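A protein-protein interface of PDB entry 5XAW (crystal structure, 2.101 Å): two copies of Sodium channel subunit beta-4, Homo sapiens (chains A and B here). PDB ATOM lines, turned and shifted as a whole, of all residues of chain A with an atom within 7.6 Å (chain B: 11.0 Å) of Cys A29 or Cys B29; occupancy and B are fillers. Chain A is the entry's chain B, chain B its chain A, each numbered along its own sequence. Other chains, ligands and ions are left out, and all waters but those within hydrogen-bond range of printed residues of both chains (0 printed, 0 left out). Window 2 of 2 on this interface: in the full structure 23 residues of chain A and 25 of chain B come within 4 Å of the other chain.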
ATOM      1  N   SER A   1      -3.919  -3.371  -6.767  1.00  0.00           N
ATOM      2  CA  SER A   1      -4.820  -3.517  -5.632  1.00  0.00           C
ATOM      3  C   SER A   1      -4.633  -2.385  -4.617  1.00  0.00           C
ATOM      4  O   SER A   1      -5.248  -1.321  -4.741  1.00  0.00           O
ATOM      5  CB  SER A   1      -4.607  -4.873  -4.957  1.00  0.00           C
ATOM      6  OG  SER A   1      -3.242  -5.060  -4.624  1.00  0.00           O
ATOM      7  N   LEU A   2      -3.778  -2.614  -3.620  1.00  0.00           N
ATOM      8  CA  LEU A   2      -3.596  -1.658  -2.537  1.00  0.00           C
ATOM      9  C   LEU A   2      -2.215  -1.832  -1.918  1.00  0.00           C
ATOM     10  O   LEU A   2      -1.737  -2.958  -1.753  1.00  0.00           O
ATOM     11  CB  LEU A   2      -4.689  -1.826  -1.472  1.00  0.00           C
ATOM     12  CG  LEU A   2      -4.394  -1.380  -0.035  1.00  0.00           C
ATOM     13  CD1 LEU A   2      -4.247   0.132   0.055  1.00  0.00           C
ATOM     14  CD2 LEU A   2      -5.480  -1.865   0.908  1.00  0.00           C
ATOM     15  N   GLU A   3      -1.586  -0.710  -1.564  1.00  0.00           N
ATOM     16  CA  GLU A   3      -0.265  -0.723  -0.952  1.00  0.00           C
ATOM     17  C   GLU A   3      -0.122   0.432   0.034  1.00  0.00           C
ATOM     18  O   GLU A   3      -0.764   1.481  -0.100  1.00  0.00           O
ATOM     19  CB  GLU A   3       0.840  -0.639  -2.003  1.00  0.00           C
ATOM     20  CG  GLU A   3       1.112   0.772  -2.467  1.00  0.00           C
ATOM     21  CD  GLU A   3       0.746   0.990  -3.921  1.00  0.00           C
ATOM     22  OE1 GLU A   3      -0.409   0.712  -4.330  1.00  0.00           O
ATOM     23  OE2 GLU A   3       1.636   1.429  -4.671  1.00  0.00           O
ATOM     24  N   SER A  27       4.508   4.217  -7.624  1.00  0.00           N
ATOM     25  CA  SER A  27       3.426   3.359  -8.065  1.00  0.00           C
ATOM     26  C   SER A  27       2.656   4.041  -9.186  1.00  0.00           C
ATOM     27  O   SER A  27       2.541   5.273  -9.233  1.00  0.00           O
ATOM     28  CB  SER A  27       2.476   3.024  -6.921  1.00  0.00           C
ATOM     29  OG  SER A  27       1.951   4.205  -6.337  1.00  0.00           O
ATOM     30  N   SER A  28       2.108   3.214 -10.071  1.00  0.00           N
ATOM     31  CA  SER A  28       1.393   3.673 -11.254  1.00  0.00           C
ATOM     32  C   SER A  28       0.103   2.884 -11.370  1.00  0.00           C
ATOM     33  O   SER A  28       0.129   1.692 -11.692  1.00  0.00           O
ATOM     34  CB  SER A  28       2.239   3.478 -12.506  1.00  0.00           C
ATOM     35  OG  SER A  28       2.664   2.123 -12.596  1.00  0.00           O
ATOM     36  N   CYS A  29      -1.022   3.539 -11.096  1.00  0.00           N
ATOM     37  CA  CYS A  29      -2.299   2.957 -11.477  1.00  0.00           C
ATOM     38  C   CYS A  29      -2.387   2.830 -12.991  1.00  0.00           C
ATOM     39  O   CYS A  29      -2.644   1.746 -13.525  1.00  0.00           O
ATOM     40  CB  CYS A  29      -3.443   3.811 -10.936  1.00  0.00           C
ATOM     41  SG  CYS A  29      -4.076   3.294  -9.299  1.00  0.00           S
ATOM     42  N   PHE A  30      -2.142   3.933 -13.697  1.00  0.00           N
ATOM     43  CA  PHE A  30      -2.140   3.984 -15.150  1.00  0.00           C
ATOM     44  C   PHE A  30      -0.930   3.248 -15.734  1.00  0.00           C
ATOM     45  O   PHE A  30      -0.124   2.658 -15.006  1.00  0.00           O
ATOM     46  CB  PHE A  30      -2.170   5.450 -15.632  1.00  0.00           C
ATOM     47  CG  PHE A  30      -0.943   6.283 -15.254  1.00  0.00           C
ATOM     48  CD1 PHE A  30      -1.086   7.380 -14.433  1.00  0.00           C
ATOM     49  CD2 PHE A  30       0.324   6.004 -15.737  1.00  0.00           C
ATOM     50  CE1 PHE A  30       0.020   8.165 -14.076  1.00  0.00           C
ATOM     51  CE2 PHE A  30       1.403   6.772 -15.395  1.00  0.00           C
ATOM     52  CZ  PHE A  30       1.261   7.849 -14.567  1.00  0.00           C
ATOM     53  N   GLY A  31      -0.794   3.323 -17.041  1.00  0.00           N
ATOM     54  CA  GLY A  31       0.398   2.799 -17.687  1.00  0.00           C
ATOM     55  C   GLY A  31       1.294   3.960 -18.071  1.00  0.00           C
ATOM     56  O   GLY A  31       0.904   4.835 -18.855  1.00  0.00           O
ATOM     57  N   PHE A  32       2.499   3.990 -17.509  1.00  0.00           N
ATOM     58  CA  PHE A  32       3.429   5.064 -17.820  1.00  0.00           C
ATOM     59  C   PHE A  32       4.378   4.648 -18.933  1.00  0.00           C
ATOM     60  O   PHE A  32       4.654   3.463 -19.152  1.00  0.00           O
ATOM     61  CB  PHE A  32       4.245   5.514 -16.594  1.00  0.00           C
ATOM     62  CG  PHE A  32       5.183   4.467 -16.036  1.00  0.00           C
ATOM     63  CD1 PHE A  32       6.462   4.302 -16.557  1.00  0.00           C
ATOM     64  CD2 PHE A  32       4.808   3.689 -14.951  1.00  0.00           C
ATOM     65  CE1 PHE A  32       7.327   3.353 -16.032  1.00  0.00           C
ATOM     66  CE2 PHE A  32       5.666   2.747 -14.428  1.00  0.00           C
ATOM     67  CZ  PHE A  32       6.926   2.577 -14.970  1.00  0.00           C
ATOM     68  N   GLU A  58       6.230   0.157 -17.437  1.00  0.00           N
ATOM     69  CA  GLU A  58       6.062  -0.595 -16.196  1.00  0.00           C
ATOM     70  C   GLU A  58       6.826  -1.907 -16.191  1.00  0.00           C
ATOM     71  O   GLU A  58       7.266  -2.362 -15.128  1.00  0.00           O
ATOM     72  CB  GLU A  58       4.593  -0.896 -15.954  1.00  0.00           C
ATOM     73  CG  GLU A  58       3.618   0.119 -16.456  1.00  0.00           C
ATOM     74  CD  GLU A  58       2.193  -0.392 -16.260  1.00  0.00           C
ATOM     75  OE1 GLU A  58       1.981  -1.639 -16.301  1.00  0.00           O
ATOM     76  OE2 GLU A  58       1.285   0.429 -15.988  1.00  0.00           O
ATOM     77  N   SER B   1      -1.406  11.206 -11.777  1.00  0.00           N
ATOM     78  CA  SER B   1      -1.943  10.303 -10.766  1.00  0.00           C
ATOM     79  C   SER B   1      -0.828   9.530 -10.077  1.00  0.00           C
ATOM     80  O   SER B   1      -1.061   8.856  -9.070  1.00  0.00           O
ATOM     81  CB  SER B   1      -2.931   9.319 -11.386  1.00  0.00           C
ATOM     82  OG  SER B   1      -2.262   8.134 -11.780  1.00  0.00           O
ATOM     83  N   LEU B   2       0.376   9.622 -10.640  1.00  0.00           N
ATOM     84  CA  LEU B   2       1.528   8.886 -10.131  1.00  0.00           C
ATOM     85  C   LEU B   2       1.864   9.317  -8.704  1.00  0.00           C
ATOM     86  O   LEU B   2       1.625  10.459  -8.303  1.00  0.00           O
ATOM     87  CB  LEU B   2       2.725   9.117 -11.055  1.00  0.00           C
ATOM     88  CG  LEU B   2       4.062   8.425 -10.795  1.00  0.00           C
ATOM     89  CD1 LEU B   2       4.080   7.022 -11.389  1.00  0.00           C
ATOM     90  CD2 LEU B   2       5.186   9.263 -11.364  1.00  0.00           C
ATOM     91  N   GLU B   3       2.440   8.388  -7.934  1.00  0.00           N
ATOM     92  CA  GLU B   3       2.748   8.622  -6.528  1.00  0.00           C
ATOM     93  C   GLU B   3       4.076   7.977  -6.147  1.00  0.00           C
ATOM     94  O   GLU B   3       4.346   6.828  -6.509  1.00  0.00           O
ATOM     95  CB  GLU B   3       1.624   8.079  -5.634  1.00  0.00           C
ATOM     96  CG  GLU B   3       1.937   8.060  -4.150  1.00  0.00           C
ATOM     97  CD  GLU B   3       1.253   6.906  -3.449  1.00  0.00           C
ATOM     98  OE1 GLU B   3       0.147   6.527  -3.894  1.00  0.00           O
ATOM     99  OE2 GLU B   3       1.821   6.373  -2.467  1.00  0.00           O
ATOM    100  N   VAL B   4       4.896   8.719  -5.403  1.00  0.00           N
ATOM    101  CA  VAL B   4       6.187   8.232  -4.928  1.00  0.00           C
ATOM    102  C   VAL B   4       6.111   7.957  -3.427  1.00  0.00           C
ATOM    103  O   VAL B   4       5.241   8.459  -2.711  1.00  0.00           O
ATOM    104  CB  VAL B   4       7.321   9.225  -5.238  1.00  0.00           C
ATOM    105  CG1 VAL B   4       7.371   9.518  -6.730  1.00  0.00           C
ATOM    106  CG2 VAL B   4       7.132  10.496  -4.433  1.00  0.00           C
ATOM    107  N   PHE B  26      -2.118   5.010   2.425  1.00  0.00           N
ATOM    108  CA  PHE B  26      -2.389   3.893   1.539  1.00  0.00           C
ATOM    109  C   PHE B  26      -3.032   4.421   0.265  1.00  0.00           C
ATOM    110  O   PHE B  26      -3.680   5.475   0.262  1.00  0.00           O
ATOM    111  CB  PHE B  26      -3.278   2.838   2.212  1.00  0.00           C
ATOM    112  CG  PHE B  26      -4.654   3.330   2.553  1.00  0.00           C
ATOM    113  CD1 PHE B  26      -4.898   3.972   3.757  1.00  0.00           C
ATOM    114  CD2 PHE B  26      -5.708   3.162   1.662  1.00  0.00           C
ATOM    115  CE1 PHE B  26      -6.164   4.439   4.070  1.00  0.00           C
ATOM    116  CE2 PHE B  26      -6.980   3.624   1.969  1.00  0.00           C
ATOM    117  CZ  PHE B  26      -7.208   4.264   3.172  1.00  0.00           C
ATOM    118  N   SER B  27      -2.834   3.680  -0.822  1.00  0.00           N
ATOM    119  CA  SER B  27      -3.323   4.082  -2.130  1.00  0.00           C
ATOM    120  C   SER B  27      -4.144   2.961  -2.751  1.00  0.00           C
ATOM    121  O   SER B  27      -3.800   1.779  -2.629  1.00  0.00           O
ATOM    122  CB  SER B  27      -2.173   4.466  -3.053  1.00  0.00           C
ATOM    123  OG  SER B  27      -1.930   5.858  -2.972  1.00  0.00           O
ATOM    124  N   SER B  28      -5.228   3.349  -3.420  1.00  0.00           N
ATOM    125  CA  SER B  28      -6.185   2.423  -4.013  1.00  0.00           C
ATOM    126  C   SER B  28      -6.164   2.587  -5.527  1.00  0.00           C
ATOM    127  O   SER B  28      -6.512   3.655  -6.038  1.00  0.00           O
ATOM    128  CB  SER B  28      -7.592   2.681  -3.469  1.00  0.00           C
ATOM    129  OG  SER B  28      -8.327   3.525  -4.345  1.00  0.00           O
ATOM    130  N   CYS B  29      -5.756   1.536  -6.239  1.00  0.00           N
ATOM    131  CA  CYS B  29      -5.898   1.519  -7.696  1.00  0.00           C
ATOM    132  C   CYS B  29      -7.321   1.148  -8.099  1.00  0.00           C
ATOM    133  O   CYS B  29      -8.102   2.002  -8.531  1.00  0.00           O
ATOM    134  CB  CYS B  29      -4.897   0.543  -8.323  1.00  0.00           C
ATOM    135  SG  CYS B  29      -3.421   1.360  -8.965  1.00  0.00           S
ATOM    136  N   PHE B  30      -7.648  -0.141  -7.993  1.00  0.00           N
ATOM    137  CA  PHE B  30      -9.008  -0.608  -8.231  1.00  0.00           C
ATOM    138  C   PHE B  30     -10.004   0.196  -7.400  1.00  0.00           C
ATOM    139  O   PHE B  30     -10.896   0.861  -7.939  1.00  0.00           O
ATOM    140  CB  PHE B  30      -9.116  -2.100  -7.890  1.00  0.00           C
ATOM    141  CG  PHE B  30      -8.318  -3.010  -8.798  1.00  0.00           C
ATOM    142  CD1 PHE B  30      -7.651  -2.518  -9.915  1.00  0.00           C
ATOM    143  CD2 PHE B  30      -8.241  -4.372  -8.526  1.00  0.00           C
ATOM    144  CE1 PHE B  30      -6.925  -3.369 -10.741  1.00  0.00           C
ATOM    145  CE2 PHE B  30      -7.518  -5.224  -9.346  1.00  0.00           C
ATOM    146  CZ  PHE B  30      -6.860  -4.725 -10.453  1.00  0.00           C
ATOM    147  N   GLY B  31      -9.828   0.170  -6.089  1.00  0.00           N
ATOM    148  CA  GLY B  31     -10.789   0.719  -5.154  1.00  0.00           C
ATOM    149  C   GLY B  31     -10.890  -0.185  -3.937  1.00  0.00           C
ATOM    150  O   GLY B  31     -10.178  -1.179  -3.816  1.00  0.00           O
ATOM    151  N   PHE B  32     -11.800   0.187  -3.038  1.00  0.00           N
ATOM    152  CA  PHE B  32     -12.011  -0.612  -1.835  1.00  0.00           C
ATOM    153  C   PHE B  32     -13.322  -0.225  -1.167  1.00  0.00           C
ATOM    154  O   PHE B  32     -13.799   0.902  -1.309  1.00  0.00           O
ATOM    155  CB  PHE B  32     -10.854  -0.458  -0.834  1.00  0.00           C
ATOM    156  CG  PHE B  32     -10.735   0.922  -0.231  1.00  0.00           C
ATOM    157  CD1 PHE B  32     -11.390   1.238   0.950  1.00  0.00           C
ATOM    158  CD2 PHE B  32      -9.952   1.892  -0.830  1.00  0.00           C
ATOM    159  CE1 PHE B  32     -11.278   2.501   1.513  1.00  0.00           C
ATOM    160  CE2 PHE B  32      -9.835   3.153  -0.273  1.00  0.00           C
ATOM    161  CZ  PHE B  32     -10.500   3.457   0.901  1.00  0.00           C
ATOM    162  N   GLU B  33     -13.892  -1.182  -0.434  1.00  0.00           N
ATOM    163  CA  GLU B  33     -14.997  -0.929   0.476  1.00  0.00           C
ATOM    164  C   GLU B  33     -14.722  -1.646   1.792  1.00  0.00           C
ATOM    165  O   GLU B  33     -14.216  -2.774   1.800  1.00  0.00           O
ATOM    166  CB  GLU B  33     -16.341  -1.379  -0.131  1.00  0.00           C
ATOM    167  CG  GLU B  33     -17.478  -1.523   0.882  1.00  0.00           C
ATOM    168  CD  GLU B  33     -18.825  -1.786   0.226  1.00  0.00           C
ATOM    169  OE1 GLU B  33     -18.841  -2.408  -0.858  1.00  0.00           O
ATOM    170  OE2 GLU B  33     -19.859  -1.362   0.795  1.00  0.00           O
ATOM    171  N   LEU B  35     -12.552  -1.207   4.456  1.00  0.00           N
ATOM    172  CA  LEU B  35     -11.178  -1.582   4.755  1.00  0.00           C
ATOM    173  C   LEU B  35     -10.946  -1.579   6.263  1.00  0.00           C
ATOM    174  O   LEU B  35     -11.470  -0.731   6.986  1.00  0.00           O
ATOM    175  CB  LEU B  35     -10.214  -0.619   4.073  1.00  0.00           C
ATOM    176  CG  LEU B  35      -8.825  -1.024   3.608  1.00  0.00           C
ATOM    177  CD1 LEU B  35      -8.927  -1.667   2.246  1.00  0.00           C
ATOM    178  CD2 LEU B  35      -7.955   0.222   3.569  1.00  0.00           C
ATOM    179  N   GLU B  58     -13.342   4.644  -0.570  1.00  0.00           N
ATOM    180  CA  GLU B  58     -12.375   5.662  -0.975  1.00  0.00           C
ATOM    181  C   GLU B  58     -12.865   7.084  -0.756  1.00  0.00           C
ATOM    182  O   GLU B  58     -12.039   7.997  -0.658  1.00  0.00           O
ATOM    183  CB  GLU B  58     -12.012   5.487  -2.447  1.00  0.00           C
ATOM    184  CG  GLU B  58     -13.151   4.956  -3.294  1.00  0.00           C
ATOM    185  CD  GLU B  58     -12.674   4.402  -4.619  1.00  0.00           C
ATOM    186  OE1 GLU B  58     -12.829   5.090  -5.651  1.00  0.00           O
ATOM    187  OE2 GLU B  58     -12.144   3.274  -4.628  1.00  0.00           O
ATOM    188  N   ASN B  83      -5.824   7.098   1.485  1.00  0.00           N
ATOM    189  CA  ASN B  83      -5.999   8.126   2.500  1.00  0.00           C
ATOM    190  C   ASN B  83      -4.951   7.986   3.606  1.00  0.00           C
ATOM    191  O   ASN B  83      -3.969   7.259   3.470  1.00  0.00           O
ATOM    192  CB  ASN B  83      -7.412   8.059   3.087  1.00  0.00           C
ATOM    193  CG  ASN B  83      -7.916   9.418   3.571  1.00  0.00           C
ATOM    194  OD1 ASN B  83      -7.591   9.869   4.681  1.00  0.00           O
ATOM    195  ND2 ASN B  83      -8.728  10.070   2.744  1.00  0.00           N
ATOM    196  N   ASN B 106      -7.857  -5.820   3.177  1.00  0.00           N
ATOM    197  CA  ASN B 106      -8.754  -5.519   2.056  1.00  0.00           C
ATOM    198  C   ASN B 106      -9.330  -6.822   1.498  1.00  0.00           C
ATOM    199  O   ASN B 106      -8.722  -7.453   0.626  1.00  0.00           O
ATOM    200  CB  ASN B 106      -8.016  -4.751   0.954  1.00  0.00           C
ATOM    201  CG  ASN B 106      -8.926  -4.338  -0.216  1.00  0.00           C
ATOM    202  OD1 ASN B 106      -9.832  -5.070  -0.619  1.00  0.00           O
ATOM    203  ND2 ASN B 106      -8.670  -3.154  -0.765  1.00  0.00           N
ATOM    204  N   HIS B 114      -1.551  -5.868   4.389  1.00  0.00           N
ATOM    205  CA  HIS B 114      -0.345  -5.083   4.192  1.00  0.00           C
ATOM    206  C   HIS B 114       0.033  -4.430   5.517  1.00  0.00           C
ATOM    207  O   HIS B 114      -0.798  -4.300   6.420  1.00  0.00           O
ATOM    208  CB  HIS B 114      -0.553  -4.024   3.104  1.00  0.00           C
ATOM    209  CG  HIS B 114      -1.354  -4.506   1.933  1.00  0.00           C
ATOM    210  ND1 HIS B 114      -2.535  -3.910   1.544  1.00  0.00           N
ATOM    211  CD2 HIS B 114      -1.141  -5.520   1.059  1.00  0.00           C
ATOM    212  CE1 HIS B 114      -3.022  -4.543   0.491  1.00  0.00           C
ATOM    213  NE2 HIS B 114      -2.194  -5.523   0.176  1.00  0.00           N
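The backbone carbonyl oxygen of Glu B3 is in hydrogen-bond range of the backbone NH of Ser A27, at 2.8 Å. The backbone carbonyl oxygen of Glu A3 sits at hydrogen-bond distance from the backbone NH of Ser B27. N of Cys B29 is in hydrogen-bond range of O of Ser A1 (3.3 Å). The side-chain sulfur of Cys B29 is disulfide-bonded to the side-chain sulfur of Cys A29, 2.1 Å away. O of Leu A2 sits close to NE2 of His B114.
The backbone carbonyl oxygen (O) of Phe B26 lies within hydrogen-bond range of the backbone NH (N) of Asn B83, 3.0 Å away. The side-chain hydroxyl (OG) of Ser A27 lies close to the side-chain carboxylate (OE2) of Glu A3, 3.3 Å away.
Ser B28 touches Ser A1 (CA to O, 3.9 Å). Leu A2 touches Phe B26. Leu A2 touches Ser B27 (CD1 to O, 3.2 Å). Leu B35 touches Leu A2. Asn B106 touches Leu A2. Phe B26 touches Glu A3. Ser A27 touches Leu B2 (O to CD1, 3.2 Å). OG of Ser B1 touches CD1 of Phe A30, 3.0 Å away. CE1 of Phe A30 touches N of Leu B2, at 3.7 Å.
Of chain B, only Ser B28 (3.9 Å) and Cys B29 (3.3 Å) come within 4 Å of Ser A1. Printed residues of chain B within 4 Å of Glu A3: Phe B26 and Ser B27. Of chain B, only Leu B2 (3.2 Å) and Glu B3 (2.8 Å) come within 4 Å of Ser A27. Ser A28 touches none of the printed residues of chain B. Cys A29 touches just one residue of chain B: Cys B29. Printed residues of chain B within 4 Å of Phe A30: Ser B1 and Leu B2. Of the printed residues of chain A, Cys B29 touches Ser A1 and Cys A29. Glu B33 touches none of the printed residues of chain A. Of the printed residues of chain A, Asn B106 touches Leu A2. Of the printed residues of chain A, His B114 touches Leu A2. The nearest printed residue of chain A that does not touch Ser B28 is Cys A29 (4.1 Å).
Of the 17 printed residues of chain B, 10 touch a printed residue of chain A.
Ser A1 touches Ser B28, but with the chains exchanged Ser A28 does not touch Ser B1 (5.8 Å). Leu A2 touches Ser B27, and with the chains exchanged Ser A27 touches Leu B2. Cys B29 touches its own counterpart, Cys A29. Phe A30 touches Leu B2, but with the chains exchanged Leu A2 does not touch Phe B30 (6.3 Å). Of the 14 pairs that touch across the chains among the printed residues, 5 have their exchanged pair printed and touching as well.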
